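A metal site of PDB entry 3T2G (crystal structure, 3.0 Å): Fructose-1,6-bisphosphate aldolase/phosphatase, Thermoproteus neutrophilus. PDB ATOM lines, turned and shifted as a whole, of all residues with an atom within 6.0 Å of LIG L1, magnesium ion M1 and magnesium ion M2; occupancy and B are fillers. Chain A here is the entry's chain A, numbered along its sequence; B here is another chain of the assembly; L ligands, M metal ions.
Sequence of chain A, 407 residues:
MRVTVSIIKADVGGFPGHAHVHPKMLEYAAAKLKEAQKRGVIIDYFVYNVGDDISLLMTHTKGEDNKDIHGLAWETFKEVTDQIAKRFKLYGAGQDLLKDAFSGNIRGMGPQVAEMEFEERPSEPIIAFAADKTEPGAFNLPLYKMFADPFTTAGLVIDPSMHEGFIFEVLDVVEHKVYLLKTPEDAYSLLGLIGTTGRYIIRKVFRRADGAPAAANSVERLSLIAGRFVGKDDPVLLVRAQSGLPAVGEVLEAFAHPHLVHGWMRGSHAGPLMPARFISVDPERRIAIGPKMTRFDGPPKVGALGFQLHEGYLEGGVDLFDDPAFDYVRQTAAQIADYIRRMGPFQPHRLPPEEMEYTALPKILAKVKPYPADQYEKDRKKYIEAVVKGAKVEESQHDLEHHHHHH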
ATOM      1  N   LYS A   9      -0.058   3.856  -0.147  1.00  0.00           N
ATOM      2  CA  LYS A   9      -0.857   2.797  -0.734  1.00  0.00           C
ATOM      3  C   LYS A   9      -1.645   2.004   0.301  1.00  0.00           C
ATOM      4  O   LYS A   9      -1.162   1.771   1.405  1.00  0.00           O
ATOM      5  CB  LYS A   9       0.100   1.873  -1.493  1.00  0.00           C
ATOM      6  CG  LYS A   9      -0.523   0.709  -2.199  1.00  0.00           C
ATOM      7  CD  LYS A   9      -0.110  -0.633  -1.567  1.00  0.00           C
ATOM      8  CE  LYS A   9      -0.806  -0.919  -0.268  1.00  0.00           C
ATOM      9  NZ  LYS A   9      -0.712  -2.339   0.161  1.00  0.00           N
ATOM     10  N   ASP A  11      -4.862  -1.335   0.749  1.00  0.00           N
ATOM     11  CA  ASP A  11      -5.987  -2.155   0.331  1.00  0.00           C
ATOM     12  C   ASP A  11      -7.142  -1.866   1.298  1.00  0.00           C
ATOM     13  O   ASP A  11      -7.047  -2.158   2.496  1.00  0.00           O
ATOM     14  CB  ASP A  11      -5.565  -3.610   0.346  1.00  0.00           C
ATOM     15  CG  ASP A  11      -6.693  -4.577  -0.034  1.00  0.00           C
ATOM     16  OD1 ASP A  11      -7.896  -4.204  -0.100  1.00  0.00           O
ATOM     17  OD2 ASP A  11      -6.346  -5.763  -0.263  1.00  0.00           O
ATOM     18  N   GLY A  14     -11.933  -5.030  -1.631  1.00  0.00           N
ATOM     19  CA  GLY A  14     -11.783  -5.738  -2.895  1.00  0.00           C
ATOM     20  C   GLY A  14     -13.114  -6.061  -3.555  1.00  0.00           C
ATOM     21  O   GLY A  14     -14.131  -6.285  -2.892  1.00  0.00           O
ATOM     22  N   GLY A  17     -13.867 -10.162  -3.829  1.00  0.00           N
ATOM     23  CA  GLY A  17     -12.769 -10.747  -3.063  1.00  0.00           C
ATOM     24  C   GLY A  17     -11.516  -9.905  -3.167  1.00  0.00           C
ATOM     25  O   GLY A  17     -11.488  -8.806  -2.677  1.00  0.00           O
ATOM     26  N   HIS A  18     -10.498 -10.417  -3.855  1.00  0.00           N
ATOM     27  CA  HIS A  18      -9.175  -9.783  -3.870  1.00  0.00           C
ATOM     28  C   HIS A  18      -8.719  -9.394  -5.294  1.00  0.00           C
ATOM     29  O   HIS A  18      -7.549  -9.051  -5.532  1.00  0.00           O
ATOM     30  CB  HIS A  18      -8.154 -10.679  -3.167  1.00  0.00           C
ATOM     31  CG  HIS A  18      -8.381 -10.817  -1.684  1.00  0.00           C
ATOM     32  ND1 HIS A  18      -8.488  -9.729  -0.843  1.00  0.00           N
ATOM     33  CD2 HIS A  18      -8.519 -11.904  -0.905  1.00  0.00           C
ATOM     34  CE1 HIS A  18      -8.690 -10.144   0.393  1.00  0.00           C
ATOM     35  NE2 HIS A  18      -8.704 -11.468   0.389  1.00  0.00           N
ATOM     36  N   VAL A  50      -3.399  -1.146  -8.629  1.00  0.00           N
ATOM     37  CA  VAL A  50      -3.032  -2.419  -9.264  1.00  0.00           C
ATOM     38  C   VAL A  50      -3.617  -3.532  -8.423  1.00  0.00           C
ATOM     39  O   VAL A  50      -3.398  -3.573  -7.219  1.00  0.00           O
ATOM     40  CB  VAL A  50      -1.512  -2.630  -9.355  1.00  0.00           C
ATOM     41  CG1 VAL A  50      -1.194  -4.045  -9.842  1.00  0.00           C
ATOM     42  CG2 VAL A  50      -0.854  -1.580 -10.278  1.00  0.00           C
ATOM     43  N   GLY A  51      -4.375  -4.427  -9.046  1.00  0.00           N
ATOM     44  CA  GLY A  51      -5.128  -5.421  -8.292  1.00  0.00           C
ATOM     45  C   GLY A  51      -6.022  -4.660  -7.313  1.00  0.00           C
ATOM     46  O   GLY A  51      -6.835  -3.818  -7.737  1.00  0.00           O
ATOM     47  N   ASP A  52      -5.847  -4.897  -6.021  1.00  0.00           N
ATOM     48  CA  ASP A  52      -6.786  -4.374  -5.053  1.00  0.00           C
ATOM     49  C   ASP A  52      -6.179  -3.334  -4.104  1.00  0.00           C
ATOM     50  O   ASP A  52      -6.752  -3.029  -3.039  1.00  0.00           O
ATOM     51  CB  ASP A  52      -7.475  -5.511  -4.293  1.00  0.00           C
ATOM     52  CG  ASP A  52      -6.523  -6.323  -3.419  1.00  0.00           C
ATOM     53  OD1 ASP A  52      -5.280  -6.164  -3.528  1.00  0.00           O
ATOM     54  OD2 ASP A  52      -7.028  -7.140  -2.606  1.00  0.00           O
ATOM     55  N   ASP A  53      -5.033  -2.778  -4.501  1.00  0.00           N
ATOM     56  CA  ASP A  53      -4.365  -1.768  -3.684  1.00  0.00           C
ATOM     57  C   ASP A  53      -4.490  -0.415  -4.327  1.00  0.00           C
ATOM     58  O   ASP A  53      -4.111  -0.237  -5.503  1.00  0.00           O
ATOM     59  CB  ASP A  53      -2.882  -2.072  -3.509  1.00  0.00           C
ATOM     60  CG  ASP A  53      -2.650  -3.424  -2.916  1.00  0.00           C
ATOM     61  OD1 ASP A  53      -2.877  -3.616  -1.685  1.00  0.00           O
ATOM     62  OD2 ASP A  53      -2.245  -4.307  -3.719  1.00  0.00           O
ATOM     63  N   TYR A  91     -14.997  -6.762  -0.159  1.00  0.00           N
ATOM     64  CA  TYR A  91     -14.254  -7.799   0.540  1.00  0.00           C
ATOM     65  C   TYR A  91     -12.954  -7.319   1.157  1.00  0.00           C
ATOM     66  O   TYR A  91     -12.088  -6.789   0.457  1.00  0.00           O
ATOM     67  CB  TYR A  91     -14.010  -9.045  -0.318  1.00  0.00           C
ATOM     68  CG  TYR A  91     -13.607 -10.212   0.551  1.00  0.00           C
ATOM     69  CD1 TYR A  91     -14.563 -11.121   0.992  1.00  0.00           C
ATOM     70  CD2 TYR A  91     -12.280 -10.369   0.971  1.00  0.00           C
ATOM     71  CE1 TYR A  91     -14.216 -12.163   1.825  1.00  0.00           C
ATOM     72  CE2 TYR A  91     -11.932 -11.411   1.813  1.00  0.00           C
ATOM     73  CZ  TYR A  91     -12.898 -12.298   2.224  1.00  0.00           C
ATOM     74  OH  TYR A  91     -12.556 -13.319   3.056  1.00  0.00           O
ATOM     75  N   GLY A  92     -12.835  -7.563   2.460  1.00  0.00           N
ATOM     76  CA  GLY A  92     -11.706  -7.095   3.271  1.00  0.00           C
ATOM     77  C   GLY A  92     -11.732  -5.586   3.294  1.00  0.00           C
ATOM     78  O   GLY A  92     -10.701  -4.938   3.127  1.00  0.00           O
ATOM     79  N   GLN A  95      -9.177  -3.171   5.106  1.00  0.00           N
ATOM     80  CA  GLN A  95      -8.202  -4.231   5.409  1.00  0.00           C
ATOM     81  C   GLN A  95      -6.916  -3.685   6.026  1.00  0.00           C
ATOM     82  O   GLN A  95      -6.525  -4.103   7.104  1.00  0.00           O
ATOM     83  CB  GLN A  95      -7.878  -5.021   4.158  1.00  0.00           C
ATOM     84  CG  GLN A  95      -7.737  -6.498   4.357  1.00  0.00           C
ATOM     85  CD  GLN A  95      -7.017  -7.110   3.189  1.00  0.00           C
ATOM     86  OE1 GLN A  95      -7.616  -7.823   2.355  1.00  0.00           O
ATOM     87  NE2 GLN A  95      -5.733  -6.792   3.084  1.00  0.00           N
ATOM     88  N   ASP A 132       0.826  -5.852  -6.934  1.00  0.00           N
ATOM     89  CA  ASP A 132      -0.204  -6.484  -6.107  1.00  0.00           C
ATOM     90  C   ASP A 132       0.109  -7.961  -5.959  1.00  0.00           C
ATOM     91  O   ASP A 132       0.728  -8.552  -6.856  1.00  0.00           O
ATOM     92  CB  ASP A 132      -1.599  -6.340  -6.707  1.00  0.00           C
ATOM     93  CG  ASP A 132      -2.683  -6.835  -5.745  1.00  0.00           C
ATOM     94  OD1 ASP A 132      -2.531  -6.626  -4.521  1.00  0.00           O
ATOM     95  OD2 ASP A 132      -3.693  -7.435  -6.194  1.00  0.00           O
ATOM     96  N   LYS A 133      -0.313  -8.538  -4.838  1.00  0.00           N
ATOM     97  CA  LYS A 133      -0.231  -9.973  -4.630  1.00  0.00           C
ATOM     98  C   LYS A 133       1.204 -10.446  -4.408  1.00  0.00           C
ATOM     99  O   LYS A 133       1.508 -11.618  -4.599  1.00  0.00           O
ATOM    100  CB  LYS A 133      -0.868 -10.711  -5.792  1.00  0.00           C
ATOM    101  CG  LYS A 133      -2.160 -11.339  -5.436  1.00  0.00           C
ATOM    102  CD  LYS A 133      -3.287 -10.374  -5.595  1.00  0.00           C
ATOM    103  CE  LYS A 133      -4.424 -10.634  -4.604  1.00  0.00           C
ATOM    104  NZ  LYS A 133      -5.295  -9.430  -4.618  1.00  0.00           N
ATOM    105  N   THR A 134       2.071  -9.535  -3.999  1.00  0.00           N
ATOM    106  CA  THR A 134       3.439  -9.843  -3.651  1.00  0.00           C
ATOM    107  C   THR A 134       3.836  -9.073  -2.397  1.00  0.00           C
ATOM    108  O   THR A 134       2.977  -8.577  -1.696  1.00  0.00           O
ATOM    109  CB  THR A 134       4.395  -9.532  -4.805  1.00  0.00           C
ATOM    110  OG1 THR A 134       5.673 -10.144  -4.558  1.00  0.00           O
ATOM    111  CG2 THR A 134       4.578  -7.991  -5.014  1.00  0.00           C
ATOM    112  N   ASP A 233       2.585  -5.734   2.814  1.00  0.00           N
ATOM    113  CA  ASP A 233       2.123  -6.434   1.640  1.00  0.00           C
ATOM    114  C   ASP A 233       2.186  -5.449   0.502  1.00  0.00           C
ATOM    115  O   ASP A 233       2.433  -4.278   0.705  1.00  0.00           O
ATOM    116  CB  ASP A 233       0.693  -6.989   1.813  1.00  0.00           C
ATOM    117  CG  ASP A 233       0.581  -8.467   1.396  1.00  0.00           C
ATOM    118  OD1 ASP A 233      -0.558  -9.007   1.404  1.00  0.00           O
ATOM    119  OD2 ASP A 233       1.639  -9.099   1.094  1.00  0.00           O
ATOM    120  N   ASP A 234       1.994  -5.973  -0.699  1.00  0.00           N
ATOM    121  CA  ASP A 234       1.911  -5.245  -1.961  1.00  0.00           C
ATOM    122  C   ASP A 234       2.563  -3.857  -1.902  1.00  0.00           C
ATOM    123  O   ASP A 234       1.900  -2.879  -1.566  1.00  0.00           O
ATOM    124  CB  ASP A 234       0.452  -5.177  -2.413  1.00  0.00           C
ATOM    125  CG  ASP A 234      -0.354  -6.419  -2.045  1.00  0.00           C
ATOM    126  OD1 ASP A 234       0.211  -7.494  -1.759  1.00  0.00           O
ATOM    127  OD2 ASP A 234      -1.598  -6.328  -2.028  1.00  0.00           O
ATOM    128  N   TRP A 264       1.392 -14.155  -4.241  1.00  0.00           N
ATOM    129  CA  TRP A 264       0.321 -14.775  -4.984  1.00  0.00           C
ATOM    130  C   TRP A 264      -0.757 -15.168  -3.977  1.00  0.00           C
ATOM    131  O   TRP A 264      -1.074 -14.408  -3.041  1.00  0.00           O
ATOM    132  CB  TRP A 264       0.800 -16.034  -5.772  1.00  0.00           C
ATOM    133  CG  TRP A 264       0.020 -16.287  -7.043  1.00  0.00           C
ATOM    134  CD1 TRP A 264      -1.196 -15.772  -7.368  1.00  0.00           C
ATOM    135  CD2 TRP A 264       0.406 -17.130  -8.150  1.00  0.00           C
ATOM    136  NE1 TRP A 264      -1.597 -16.213  -8.617  1.00  0.00           N
ATOM    137  CE2 TRP A 264      -0.635 -17.056  -9.116  1.00  0.00           C
ATOM    138  CE3 TRP A 264       1.518 -17.952  -8.423  1.00  0.00           C
ATOM    139  CZ2 TRP A 264      -0.594 -17.764 -10.340  1.00  0.00           C
ATOM    140  CZ3 TRP A 264       1.554 -18.652  -9.646  1.00  0.00           C
ATOM    141  CH2 TRP A 264       0.507 -18.547 -10.582  1.00  0.00           C
ATOM    142  N   MET A 265      -1.276 -16.378  -4.140  1.00  0.00           N
ATOM    143  CA  MET A 265      -2.490 -16.795  -3.483  1.00  0.00           C
ATOM    144  C   MET A 265      -2.284 -17.125  -2.039  1.00  0.00           C
ATOM    145  O   MET A 265      -1.504 -18.034  -1.709  1.00  0.00           O
ATOM    146  CB  MET A 265      -3.040 -18.017  -4.189  1.00  0.00           C
ATOM    147  CG  MET A 265      -3.887 -18.916  -3.332  1.00  0.00           C
ATOM    148  SD  MET A 265      -5.519 -18.272  -2.936  1.00  0.00           S
ATOM    149  CE  MET A 265      -6.255 -17.911  -4.540  1.00  0.00           C
ATOM    150  N   ARG A 266      -3.011 -16.384  -1.202  1.00  0.00           N
ATOM    151  CA  ARG A 266      -2.964 -16.497   0.260  1.00  0.00           C
ATOM    152  C   ARG A 266      -1.629 -16.105   0.895  1.00  0.00           C
ATOM    153  O   ARG A 266      -1.333 -16.487   2.020  1.00  0.00           O
ATOM    154  CB  ARG A 266      -3.405 -17.857   0.732  1.00  0.00           C
ATOM    155  CG  ARG A 266      -4.794 -18.181   0.286  1.00  0.00           C
ATOM    156  CD  ARG A 266      -5.118 -19.614   0.607  1.00  0.00           C
ATOM    157  NE  ARG A 266      -6.473 -19.953   0.197  1.00  0.00           N
ATOM    158  CZ  ARG A 266      -7.530 -19.928   0.997  1.00  0.00           C
ATOM    159  NH1 ARG A 266      -7.404 -19.604   2.281  1.00  0.00           N
ATOM    160  NH2 ARG A 266      -8.719 -20.255   0.495  1.00  0.00           N
ATOM    161  N   GLY A 267      -0.866 -15.295   0.159  1.00  0.00           N
ATOM    162  CA  GLY A 267       0.434 -14.799   0.602  1.00  0.00           C
ATOM    163  C   GLY A 267       1.409 -15.923   0.908  1.00  0.00           C
ATOM    164  O   GLY A 267       2.323 -15.738   1.711  1.00  0.00           O
ATOM    165  N   SER A 268       1.222 -17.054   0.234  1.00  0.00           N
ATOM    166  CA  SER A 268       1.912 -18.279   0.596  1.00  0.00           C
ATOM    167  C   SER A 268       2.527 -19.079  -0.554  1.00  0.00           C
ATOM    168  O   SER A 268       2.962 -20.246  -0.372  1.00  0.00           O
ATOM    169  CB  SER A 268       0.966 -19.163   1.410  1.00  0.00           C
ATOM    170  OG  SER A 268       0.369 -18.375   2.416  1.00  0.00           O
ATOM    171  N   PHE A 296      -5.772 -18.139  -9.652  1.00  0.00           N
ATOM    172  CA  PHE A 296      -5.108 -18.309  -8.380  1.00  0.00           C
ATOM    173  C   PHE A 296      -4.850 -17.002  -7.626  1.00  0.00           C
ATOM    174  O   PHE A 296      -4.014 -16.989  -6.739  1.00  0.00           O
ATOM    175  CB  PHE A 296      -3.789 -19.077  -8.581  1.00  0.00           C
ATOM    176  CG  PHE A 296      -3.386 -19.930  -7.391  1.00  0.00           C
ATOM    177  CD1 PHE A 296      -4.297 -20.804  -6.797  1.00  0.00           C
ATOM    178  CD2 PHE A 296      -2.094 -19.878  -6.894  1.00  0.00           C
ATOM    179  CE1 PHE A 296      -3.950 -21.588  -5.723  1.00  0.00           C
ATOM    180  CE2 PHE A 296      -1.726 -20.671  -5.823  1.00  0.00           C
ATOM    181  CZ  PHE A 296      -2.663 -21.528  -5.226  1.00  0.00           C
ATOM    182  N   ASP A 297      -5.593 -15.925  -7.941  1.00  0.00           N
ATOM    183  CA  ASP A 297      -5.374 -14.583  -7.354  1.00  0.00           C
ATOM    184  C   ASP A 297      -4.080 -13.918  -7.803  1.00  0.00           C
ATOM    185  O   ASP A 297      -3.324 -13.373  -6.989  1.00  0.00           O
ATOM    186  CB  ASP A 297      -5.382 -14.578  -5.827  1.00  0.00           C
ATOM    187  CG  ASP A 297      -6.750 -14.635  -5.262  1.00  0.00           C
ATOM    188  OD1 ASP A 297      -7.727 -14.540  -6.036  1.00  0.00           O
ATOM    189  OD2 ASP A 297      -6.849 -14.790  -4.026  1.00  0.00           O
ATOM    190  N   ALA B 247     -11.136 -19.249  -2.241  1.00  0.00           N
ATOM    191  CA  ALA B 247     -10.830 -17.884  -2.658  1.00  0.00           C
ATOM    192  C   ALA B 247     -11.402 -17.719  -4.059  1.00  0.00           C
ATOM    193  O   ALA B 247     -11.624 -18.720  -4.773  1.00  0.00           O
ATOM    194  CB  ALA B 247      -9.335 -17.652  -2.654  1.00  0.00           C
HETATM  195  P1  LIG L   1      -3.823  -8.796  -1.049  1.00  0.00           P
HETATM  196  O1  LIG L   1      -2.459  -8.791  -0.400  1.00  0.00           O
HETATM  197  O2  LIG L   1      -3.796  -8.297  -2.472  1.00  0.00           O
HETATM  198  O3  LIG L   1      -4.973  -8.246  -0.227  1.00  0.00           O
HETATM  199  O4  LIG L   1      -4.118 -10.378  -1.203  1.00  0.00           O
HETATM  200  C1  LIG L   1      -4.305 -11.207  -0.051  1.00  0.00           C
HETATM  201  C2  LIG L   1      -4.260 -12.655  -0.426  1.00  0.00           C
HETATM  202  O5  LIG L   1      -3.476 -13.392   0.140  1.00  0.00           O
HETATM  203  C3  LIG L   1      -5.200 -13.168  -1.482  1.00  0.00           C
HETATM  204  O6  LIG L   1      -4.871 -14.492  -1.884  1.00  0.00           O
HETATM  205  P1  LG2 L   2     -10.035 -15.402   3.019  1.00  0.00           P
HETATM  206  O1  LG2 L   2     -11.247 -15.756   2.196  1.00  0.00           O
HETATM  207  O2  LG2 L   2      -9.371 -16.543   3.748  1.00  0.00           O
HETATM  208  O3  LG2 L   2     -10.122 -14.087   3.774  1.00  0.00           O
HETATM  209  O4  LG2 L   2      -8.963 -15.103   1.875  1.00  0.00           O
HETATM  210  C1  LG2 L   2      -8.723 -16.014   0.808  1.00  0.00           C
HETATM  211  C2  LG2 L   2      -7.874 -15.183  -0.108  1.00  0.00           C
HETATM  212  O5  LG2 L   2      -8.257 -14.883  -1.224  1.00  0.00           O
HETATM  213  C3  LG2 L   2      -6.564 -14.674   0.424  1.00  0.00           C
HETATM  214  O6  LG2 L   2      -6.435 -14.884   1.845  1.00  0.00           O
HETATM  215 MG    MG M   1      -7.314  -7.709  -0.421  1.00  0.00          MG
HETATM  216 MG    MG M   2      -3.577  -6.279  -2.426  1.00  0.00          MG
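The side-chain carboxylate (OD1) of Asp 233 sits close to an oxygen (O1) of LIG L1 (2.6 Å). An oxygen (O6) of LIG L1 lies within hydrogen-bond range of the backbone NH (N) of Arg 266, at 2.7 Å. The side-chain amino group (NZ) of Lys 133 lies close to an oxygen (O2) of LIG L1, at 2.9 Å. OD2 of Asp 297 is in hydrogen-bond range of O6 of LIG L1 (2.9 Å). An oxygen (O5) of LIG L1 lies within hydrogen-bond range of the backbone NH of Gly 267 (3.2 Å). The guanidinium group (NH1) of Arg 266 lies within salt-bridge range of an oxygen (O2) of LG2 L2 (3.9 Å). OH of Tyr 91 lies within hydrogen-bond range of O3 of LG2 L2, at 2.7 Å.
An oxygen (O6) of LIG L1 lies close to an oxygen (O5) of LG2 L2 (3.5 Å).
OD2 of Asp 234 lies close to OD2 of Asp 53, at 2.7 Å. The side-chain carboxylate (OD1) of Asp 234 sits at hydrogen-bond distance from the backbone NH (N) of Lys 133 (3.3 Å). O of Asp 234 sits close to NZ of Lys 9 (3.2 Å). The side-chain amino group of Lys 133 sits close to the side-chain carboxylate of Asp 52 (3.4 Å). The side-chain carboxylate (OD1) of Asp 132 sits close to the side-chain carboxylate (OD2) of Asp 53, at 2.5 Å. The side-chain amino group (NZ) of Lys 9 is in salt-bridge range of the side-chain carboxylate (OD1) of Asp 53 (3.1 Å). The guanidinium group (NE) of Arg 266 sits close to the side-chain sulfur (SD) of Met 265 (3.7 Å). The indole nitrogen (NE1) of Trp 264 lies close to the backbone carbonyl oxygen (O) of Phe 296 (3.2 Å).
Merely in contact with LIG L1: Met 265 (3.7 Å) and Trp 264 (3.97 Å). Within 4 Å of LIG L1: Asp 11, His 18, Asp 52, Gln 95, Asp 132, Lys 133, Asp 233, Asp 234, Trp 264, Met 265, Arg 266, Gly 267 and Asp 297.
Within 4 Å of magnesium ion M1: Asp 11, His 18, Asp 52 and Gln 95. The nearest printed residue that does not touch magnesium ion M1 is Gly 17 (4.9 Å).
Five residues have an atom within 4 Å of magnesium ion M2: Asp 11, Asp 52, Asp 53, Asp 132 and Asp 234. Along chain A the residues within 4 Å of magnesium ion M2 span positions 11 to 234. The nearest printed residue that does not touch magnesium ion M2 is Lys 133 (4.2 Å).
Magnesium ion M1 is bound by OD2 of Asp 11, at 2.2 Å. Magnesium ion M1 is bound by OD2 of Asp 52, at 2.3 Å. A ring nitrogen (ND1) of His 18 binds magnesium ion M1. Magnesium ion M1 is bound by O3 of LIG L1 (2.4 Å). Slightly farther from magnesium ion M1 lies the side-chain amide oxygen (OE1) of Gln 95 (2.8 Å).
Magnesium ion M2 is bound by OD2 of Asp 234 (2.0 Å), O2 of LIG L1 (2.0 Å), OD1 of Asp 52 (2.0 Å) and OD1 of Asp 132 (2.4 Å). Magnesium ion M2 has four donor atoms within binding distance. Slightly farther from magnesium ion M2 lies OD2 of Asp 53 (2.7 Å).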
